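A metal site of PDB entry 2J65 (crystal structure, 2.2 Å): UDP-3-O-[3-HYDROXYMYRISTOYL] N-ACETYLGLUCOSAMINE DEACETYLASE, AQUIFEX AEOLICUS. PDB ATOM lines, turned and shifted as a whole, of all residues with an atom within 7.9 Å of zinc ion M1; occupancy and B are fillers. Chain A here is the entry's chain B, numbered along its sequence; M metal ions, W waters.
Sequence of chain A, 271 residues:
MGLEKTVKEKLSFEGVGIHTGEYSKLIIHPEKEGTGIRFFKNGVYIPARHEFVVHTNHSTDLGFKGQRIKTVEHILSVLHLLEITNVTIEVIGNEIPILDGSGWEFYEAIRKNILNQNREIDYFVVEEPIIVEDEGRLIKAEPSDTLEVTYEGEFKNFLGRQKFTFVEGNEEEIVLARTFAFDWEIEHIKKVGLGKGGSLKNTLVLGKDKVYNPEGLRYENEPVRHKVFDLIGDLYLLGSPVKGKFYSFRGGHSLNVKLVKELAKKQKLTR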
ATOM      1  N   HIS A  58      11.254 -11.976  -8.835  1.00  0.00           N
ATOM      2  CA  HIS A  58       9.863 -12.134  -8.365  1.00  0.00           C
ATOM      3  C   HIS A  58       8.841 -11.420  -9.278  1.00  0.00           C
ATOM      4  O   HIS A  58       7.705 -11.145  -8.873  1.00  0.00           O
ATOM      5  CB  HIS A  58       9.739 -11.669  -6.908  1.00  0.00           C
ATOM      6  CG  HIS A  58      10.666 -12.387  -5.975  1.00  0.00           C
ATOM      7  ND1 HIS A  58      10.382 -13.639  -5.457  1.00  0.00           N
ATOM      8  CD2 HIS A  58      11.891 -12.061  -5.503  1.00  0.00           C
ATOM      9  CE1 HIS A  58      11.383 -14.033  -4.692  1.00  0.00           C
ATOM     10  NE2 HIS A  58      12.303 -13.087  -4.688  1.00  0.00           N
ATOM     11  N   SER A  59       9.272 -11.131 -10.502  1.00  0.00           N
ATOM     12  CA  SER A  59       8.467 -10.494 -11.548  1.00  0.00           C
ATOM     13  C   SER A  59       9.364 -10.348 -12.744  1.00  0.00           C
ATOM     14  O   SER A  59      10.584 -10.538 -12.626  1.00  0.00           O
ATOM     15  CB  SER A  59       7.932  -9.103 -11.118  1.00  0.00           C
ATOM     16  OG  SER A  59       8.945  -8.249 -10.605  1.00  0.00           O
ATOM     17  N   THR A  71       6.773  -5.869 -13.312  1.00  0.00           N
ATOM     18  CA  THR A  71       5.628  -6.792 -13.360  1.00  0.00           C
ATOM     19  C   THR A  71       4.809  -6.668 -14.643  1.00  0.00           C
ATOM     20  O   THR A  71       3.603  -6.428 -14.595  1.00  0.00           O
ATOM     21  CB  THR A  71       4.714  -6.649 -12.093  1.00  0.00           C
ATOM     22  OG1 THR A  71       5.521  -6.390 -10.948  1.00  0.00           O
ATOM     23  CG2 THR A  71       3.909  -7.922 -11.843  1.00  0.00           C
ATOM     24  N   GLU A  73       4.441  -9.159 -16.820  1.00  0.00           N
ATOM     25  CA  GLU A  73       4.076 -10.499 -17.302  1.00  0.00           C
ATOM     26  C   GLU A  73       2.579 -10.735 -17.612  1.00  0.00           C
ATOM     27  O   GLU A  73       2.258 -11.479 -18.533  1.00  0.00           O
ATOM     28  CB  GLU A  73       4.627 -11.619 -16.392  1.00  0.00           C
ATOM     29  CG  GLU A  73       4.253 -11.525 -14.901  1.00  0.00           C
ATOM     30  CD  GLU A  73       5.322 -10.834 -14.013  1.00  0.00           C
ATOM     31  OE1 GLU A  73       6.065  -9.957 -14.485  1.00  0.00           O
ATOM     32  OE2 GLU A  73       5.389 -11.190 -12.819  1.00  0.00           O
ATOM     33  N   HIS A  74       1.691 -10.108 -16.858  1.00  0.00           N
ATOM     34  CA  HIS A  74       0.260 -10.403 -16.970  1.00  0.00           C
ATOM     35  C   HIS A  74      -0.434  -9.636 -18.105  1.00  0.00           C
ATOM     36  O   HIS A  74      -1.200 -10.225 -18.870  1.00  0.00           O
ATOM     37  CB  HIS A  74      -0.486 -10.205 -15.632  1.00  0.00           C
ATOM     38  CG  HIS A  74       0.043 -11.055 -14.514  1.00  0.00           C
ATOM     39  ND1 HIS A  74      -0.205 -10.776 -13.185  1.00  0.00           N
ATOM     40  CD2 HIS A  74       0.838 -12.160 -14.522  1.00  0.00           C
ATOM     41  CE1 HIS A  74       0.399 -11.670 -12.427  1.00  0.00           C
ATOM     42  NE2 HIS A  74       1.032 -12.522 -13.209  1.00  0.00           N
ATOM     43  N   ILE A  98      -1.595  -4.662 -10.234  1.00  0.00           N
ATOM     44  CA  ILE A  98      -1.810  -6.115 -10.128  1.00  0.00           C
ATOM     45  C   ILE A  98      -3.288  -6.526 -10.252  1.00  0.00           C
ATOM     46  O   ILE A  98      -3.596  -7.630 -10.693  1.00  0.00           O
ATOM     47  CB  ILE A  98      -1.162  -6.708  -8.830  1.00  0.00           C
ATOM     48  CG1 ILE A  98      -1.183  -8.254  -8.860  1.00  0.00           C
ATOM     49  CG2 ILE A  98      -1.818  -6.161  -7.573  1.00  0.00           C
ATOM     50  CD1 ILE A  98      -0.184  -8.876  -9.831  1.00  0.00           C
ATOM     51  N   GLY A 101      -4.687 -10.109  -9.341  1.00  0.00           N
ATOM     52  CA  GLY A 101      -3.600 -11.094  -9.516  1.00  0.00           C
ATOM     53  C   GLY A 101      -3.724 -11.991 -10.751  1.00  0.00           C
ATOM     54  O   GLY A 101      -2.844 -12.812 -10.996  1.00  0.00           O
ATOM     55  N   SER A 102      -4.812 -11.848 -11.514  1.00  0.00           N
ATOM     56  CA  SER A 102      -4.995 -12.619 -12.768  1.00  0.00           C
ATOM     57  C   SER A 102      -5.010 -11.682 -13.981  1.00  0.00           C
ATOM     58  O   SER A 102      -4.797 -10.486 -13.845  1.00  0.00           O
ATOM     59  CB  SER A 102      -6.285 -13.461 -12.721  1.00  0.00           C
ATOM     60  OG  SER A 102      -7.461 -12.659 -12.825  1.00  0.00           O
ATOM     61  N   ALA A 177      -6.727 -17.413 -13.481  1.00  0.00           N
ATOM     62  CA  ALA A 177      -5.793 -17.970 -12.514  1.00  0.00           C
ATOM     63  C   ALA A 177      -4.868 -16.896 -11.890  1.00  0.00           C
ATOM     64  O   ALA A 177      -4.105 -16.208 -12.587  1.00  0.00           O
ATOM     65  CB  ALA A 177      -4.988 -19.118 -13.129  1.00  0.00           C
ATOM     66  N   ARG A 178      -4.947 -16.774 -10.568  1.00  0.00           N
ATOM     67  CA  ARG A 178      -4.216 -15.722  -9.860  1.00  0.00           C
ATOM     68  C   ARG A 178      -2.808 -16.102  -9.449  1.00  0.00           C
ATOM     69  O   ARG A 178      -2.459 -17.291  -9.294  1.00  0.00           O
ATOM     70  CB  ARG A 178      -4.977 -15.280  -8.627  1.00  0.00           C
ATOM     71  CG  ARG A 178      -6.399 -14.942  -8.904  1.00  0.00           C
ATOM     72  CD  ARG A 178      -6.991 -14.234  -7.728  1.00  0.00           C
ATOM     73  NE  ARG A 178      -7.665 -15.119  -6.801  1.00  0.00           N
ATOM     74  CZ  ARG A 178      -7.858 -14.836  -5.517  1.00  0.00           C
ATOM     75  NH1 ARG A 178      -8.496 -15.698  -4.731  1.00  0.00           N
ATOM     76  NH2 ARG A 178      -7.384 -13.701  -4.996  1.00  0.00           N
ATOM     77  N   THR A 179      -1.993 -15.061  -9.265  1.00  0.00           N
ATOM     78  CA  THR A 179      -0.661 -15.179  -8.731  1.00  0.00           C
ATOM     79  C   THR A 179      -0.715 -15.716  -7.292  1.00  0.00           C
ATOM     80  O   THR A 179      -1.718 -15.564  -6.604  1.00  0.00           O
ATOM     81  CB  THR A 179       0.120 -13.836  -8.831  1.00  0.00           C
ATOM     82  OG1 THR A 179       1.484 -14.056  -8.463  1.00  0.00           O
ATOM     83  CG2 THR A 179      -0.486 -12.768  -7.930  1.00  0.00           C
ATOM     84  N   PHE A 180       0.354 -16.372  -6.866  1.00  0.00           N
ATOM     85  CA  PHE A 180       0.322 -17.065  -5.584  1.00  0.00           C
ATOM     86  C   PHE A 180       1.653 -16.952  -4.859  1.00  0.00           C
ATOM     87  O   PHE A 180       2.694 -16.696  -5.470  1.00  0.00           O
ATOM     88  CB  PHE A 180      -0.101 -18.538  -5.766  1.00  0.00           C
ATOM     89  CG  PHE A 180       0.851 -19.357  -6.587  1.00  0.00           C
ATOM     90  CD1 PHE A 180       1.757 -20.226  -5.968  1.00  0.00           C
ATOM     91  CD2 PHE A 180       0.853 -19.253  -7.984  1.00  0.00           C
ATOM     92  CE1 PHE A 180       2.647 -20.966  -6.732  1.00  0.00           C
ATOM     93  CE2 PHE A 180       1.734 -19.994  -8.742  1.00  0.00           C
ATOM     94  CZ  PHE A 180       2.639 -20.849  -8.122  1.00  0.00           C
ATOM     95  N   HIS A 226      -1.744 -20.628 -13.395  1.00  0.00           N
ATOM     96  CA  HIS A 226      -1.105 -19.315 -13.369  1.00  0.00           C
ATOM     97  C   HIS A 226       0.309 -19.333 -13.945  1.00  0.00           C
ATOM     98  O   HIS A 226       0.714 -18.379 -14.619  1.00  0.00           O
ATOM     99  CB  HIS A 226      -1.089 -18.678 -11.982  1.00  0.00           C
ATOM    100  CG  HIS A 226      -0.595 -17.270 -12.005  1.00  0.00           C
ATOM    101  ND1 HIS A 226      -1.430 -16.196 -12.253  1.00  0.00           N
ATOM    102  CD2 HIS A 226       0.655 -16.760 -11.908  1.00  0.00           C
ATOM    103  CE1 HIS A 226      -0.716 -15.087 -12.261  1.00  0.00           C
ATOM    104  NE2 HIS A 226       0.551 -15.399 -12.066  1.00  0.00           N
ATOM    105  N   LYS A 227       1.062 -20.400 -13.692  1.00  0.00           N
ATOM    106  CA  LYS A 227       2.407 -20.534 -14.257  1.00  0.00           C
ATOM    107  C   LYS A 227       2.438 -20.623 -15.791  1.00  0.00           C
ATOM    108  O   LYS A 227       3.382 -20.119 -16.445  1.00  0.00           O
ATOM    109  CB  LYS A 227       3.145 -21.713 -13.629  1.00  0.00           C
ATOM    110  CG  LYS A 227       3.622 -21.465 -12.197  1.00  0.00           C
ATOM    111  CD  LYS A 227       4.940 -20.703 -12.167  1.00  0.00           C
ATOM    112  CE  LYS A 227       5.393 -20.474 -10.721  1.00  0.00           C
ATOM    113  NZ  LYS A 227       6.819 -20.003 -10.643  1.00  0.00           N
ATOM    114  N   PHE A 229       0.072 -19.164 -17.621  1.00  0.00           N
ATOM    115  CA  PHE A 229      -0.227 -17.760 -17.900  1.00  0.00           C
ATOM    116  C   PHE A 229       1.055 -16.893 -17.879  1.00  0.00           C
ATOM    117  O   PHE A 229       1.325 -16.170 -18.824  1.00  0.00           O
ATOM    118  CB  PHE A 229      -1.298 -17.260 -16.925  1.00  0.00           C
ATOM    119  CG  PHE A 229      -1.740 -15.829 -17.175  1.00  0.00           C
ATOM    120  CD1 PHE A 229      -2.558 -15.518 -18.256  1.00  0.00           C
ATOM    121  CD2 PHE A 229      -1.335 -14.817 -16.330  1.00  0.00           C
ATOM    122  CE1 PHE A 229      -2.966 -14.216 -18.489  1.00  0.00           C
ATOM    123  CE2 PHE A 229      -1.757 -13.497 -16.543  1.00  0.00           C
ATOM    124  CZ  PHE A 229      -2.578 -13.207 -17.633  1.00  0.00           C
ATOM    125  N   ASP A 230       1.853 -16.994 -16.827  1.00  0.00           N
ATOM    126  CA  ASP A 230       3.156 -16.318 -16.752  1.00  0.00           C
ATOM    127  C   ASP A 230       4.083 -16.590 -17.961  1.00  0.00           C
ATOM    128  O   ASP A 230       4.670 -15.657 -18.528  1.00  0.00           O
ATOM    129  CB  ASP A 230       3.906 -16.774 -15.501  1.00  0.00           C
ATOM    130  CG  ASP A 230       3.509 -16.026 -14.238  1.00  0.00           C
ATOM    131  OD1 ASP A 230       2.768 -15.000 -14.298  1.00  0.00           O
ATOM    132  OD2 ASP A 230       3.973 -16.475 -13.163  1.00  0.00           O
ATOM    133  N   LEU A 231       4.234 -17.874 -18.322  1.00  0.00           N
ATOM    134  CA  LEU A 231       5.144 -18.243 -19.417  1.00  0.00           C
ATOM    135  C   LEU A 231       4.710 -17.640 -20.755  1.00  0.00           C
ATOM    136  O   LEU A 231       5.556 -17.184 -21.535  1.00  0.00           O
ATOM    137  CB  LEU A 231       5.292 -19.769 -19.533  1.00  0.00           C
ATOM    138  CG  LEU A 231       6.089 -20.390 -20.685  1.00  0.00           C
ATOM    139  CD1 LEU A 231       7.504 -19.807 -20.853  1.00  0.00           C
ATOM    140  CD2 LEU A 231       6.183 -21.893 -20.490  1.00  0.00           C
ATOM    141  N   ASP A 234       5.877 -13.993 -20.741  1.00  0.00           N
ATOM    142  CA  ASP A 234       7.319 -13.963 -20.982  1.00  0.00           C
ATOM    143  C   ASP A 234       7.709 -14.327 -22.430  1.00  0.00           C
ATOM    144  O   ASP A 234       8.665 -13.759 -22.975  1.00  0.00           O
ATOM    145  CB  ASP A 234       8.061 -14.865 -19.976  1.00  0.00           C
ATOM    146  CG  ASP A 234       8.005 -14.323 -18.523  1.00  0.00           C
ATOM    147  OD1 ASP A 234       7.856 -13.086 -18.338  1.00  0.00           O
ATOM    148  OD2 ASP A 234       8.095 -15.144 -17.571  1.00  0.00           O
ATOM    149  N   HIS A 253      10.033 -17.113 -13.960  1.00  0.00           N
ATOM    150  CA  HIS A 253      10.436 -15.995 -14.832  1.00  0.00           C
ATOM    151  C   HIS A 253      11.898 -16.038 -15.305  1.00  0.00           C
ATOM    152  O   HIS A 253      12.165 -15.785 -16.475  1.00  0.00           O
ATOM    153  CB  HIS A 253      10.129 -14.636 -14.190  1.00  0.00           C
ATOM    154  CG  HIS A 253       8.677 -14.406 -13.912  1.00  0.00           C
ATOM    155  ND1 HIS A 253       7.711 -14.503 -14.887  1.00  0.00           N
ATOM    156  CD2 HIS A 253       8.030 -14.064 -12.773  1.00  0.00           C
ATOM    157  CE1 HIS A 253       6.523 -14.266 -14.349  1.00  0.00           C
ATOM    158  NE2 HIS A 253       6.694 -13.972 -13.077  1.00  0.00           N
HETATM  159 ZN    ZN M   1       2.066 -14.153 -12.603  1.00  0.00          ZN
HETATM  160 ZN    ZN M   2       5.181 -13.131 -11.890  1.00  0.00          ZN
HETATM  161  O   HOH W   1       3.087 -13.686 -10.663  1.00  0.00           O
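ND1 of His 226 sits at hydrogen-bond distance from N of Thr 179 (3.2 Å).
The backbone carbonyl oxygen (O) of Arg 178 lies close to a ring nitrogen (ND1) of His 226, at 3.3 Å.
The backbone carbonyl oxygen (O) of Ala 177 is in hydrogen-bond range of a ring nitrogen (ND1) of His 226 (2.7 Å).
Zinc ion M1 is bound by the side-chain carboxylate (OD1) of Asp 230.
NE2 of His 74 is bound to zinc ion M1, at 2.0 Å.
A ring nitrogen (NE2) of His 226 is bound to zinc ion M1.
Zinc ion M1 is bound by water W1.
The nearest printed residue that does not touch zinc ion M1 is Glu 73 (4.1 Å).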
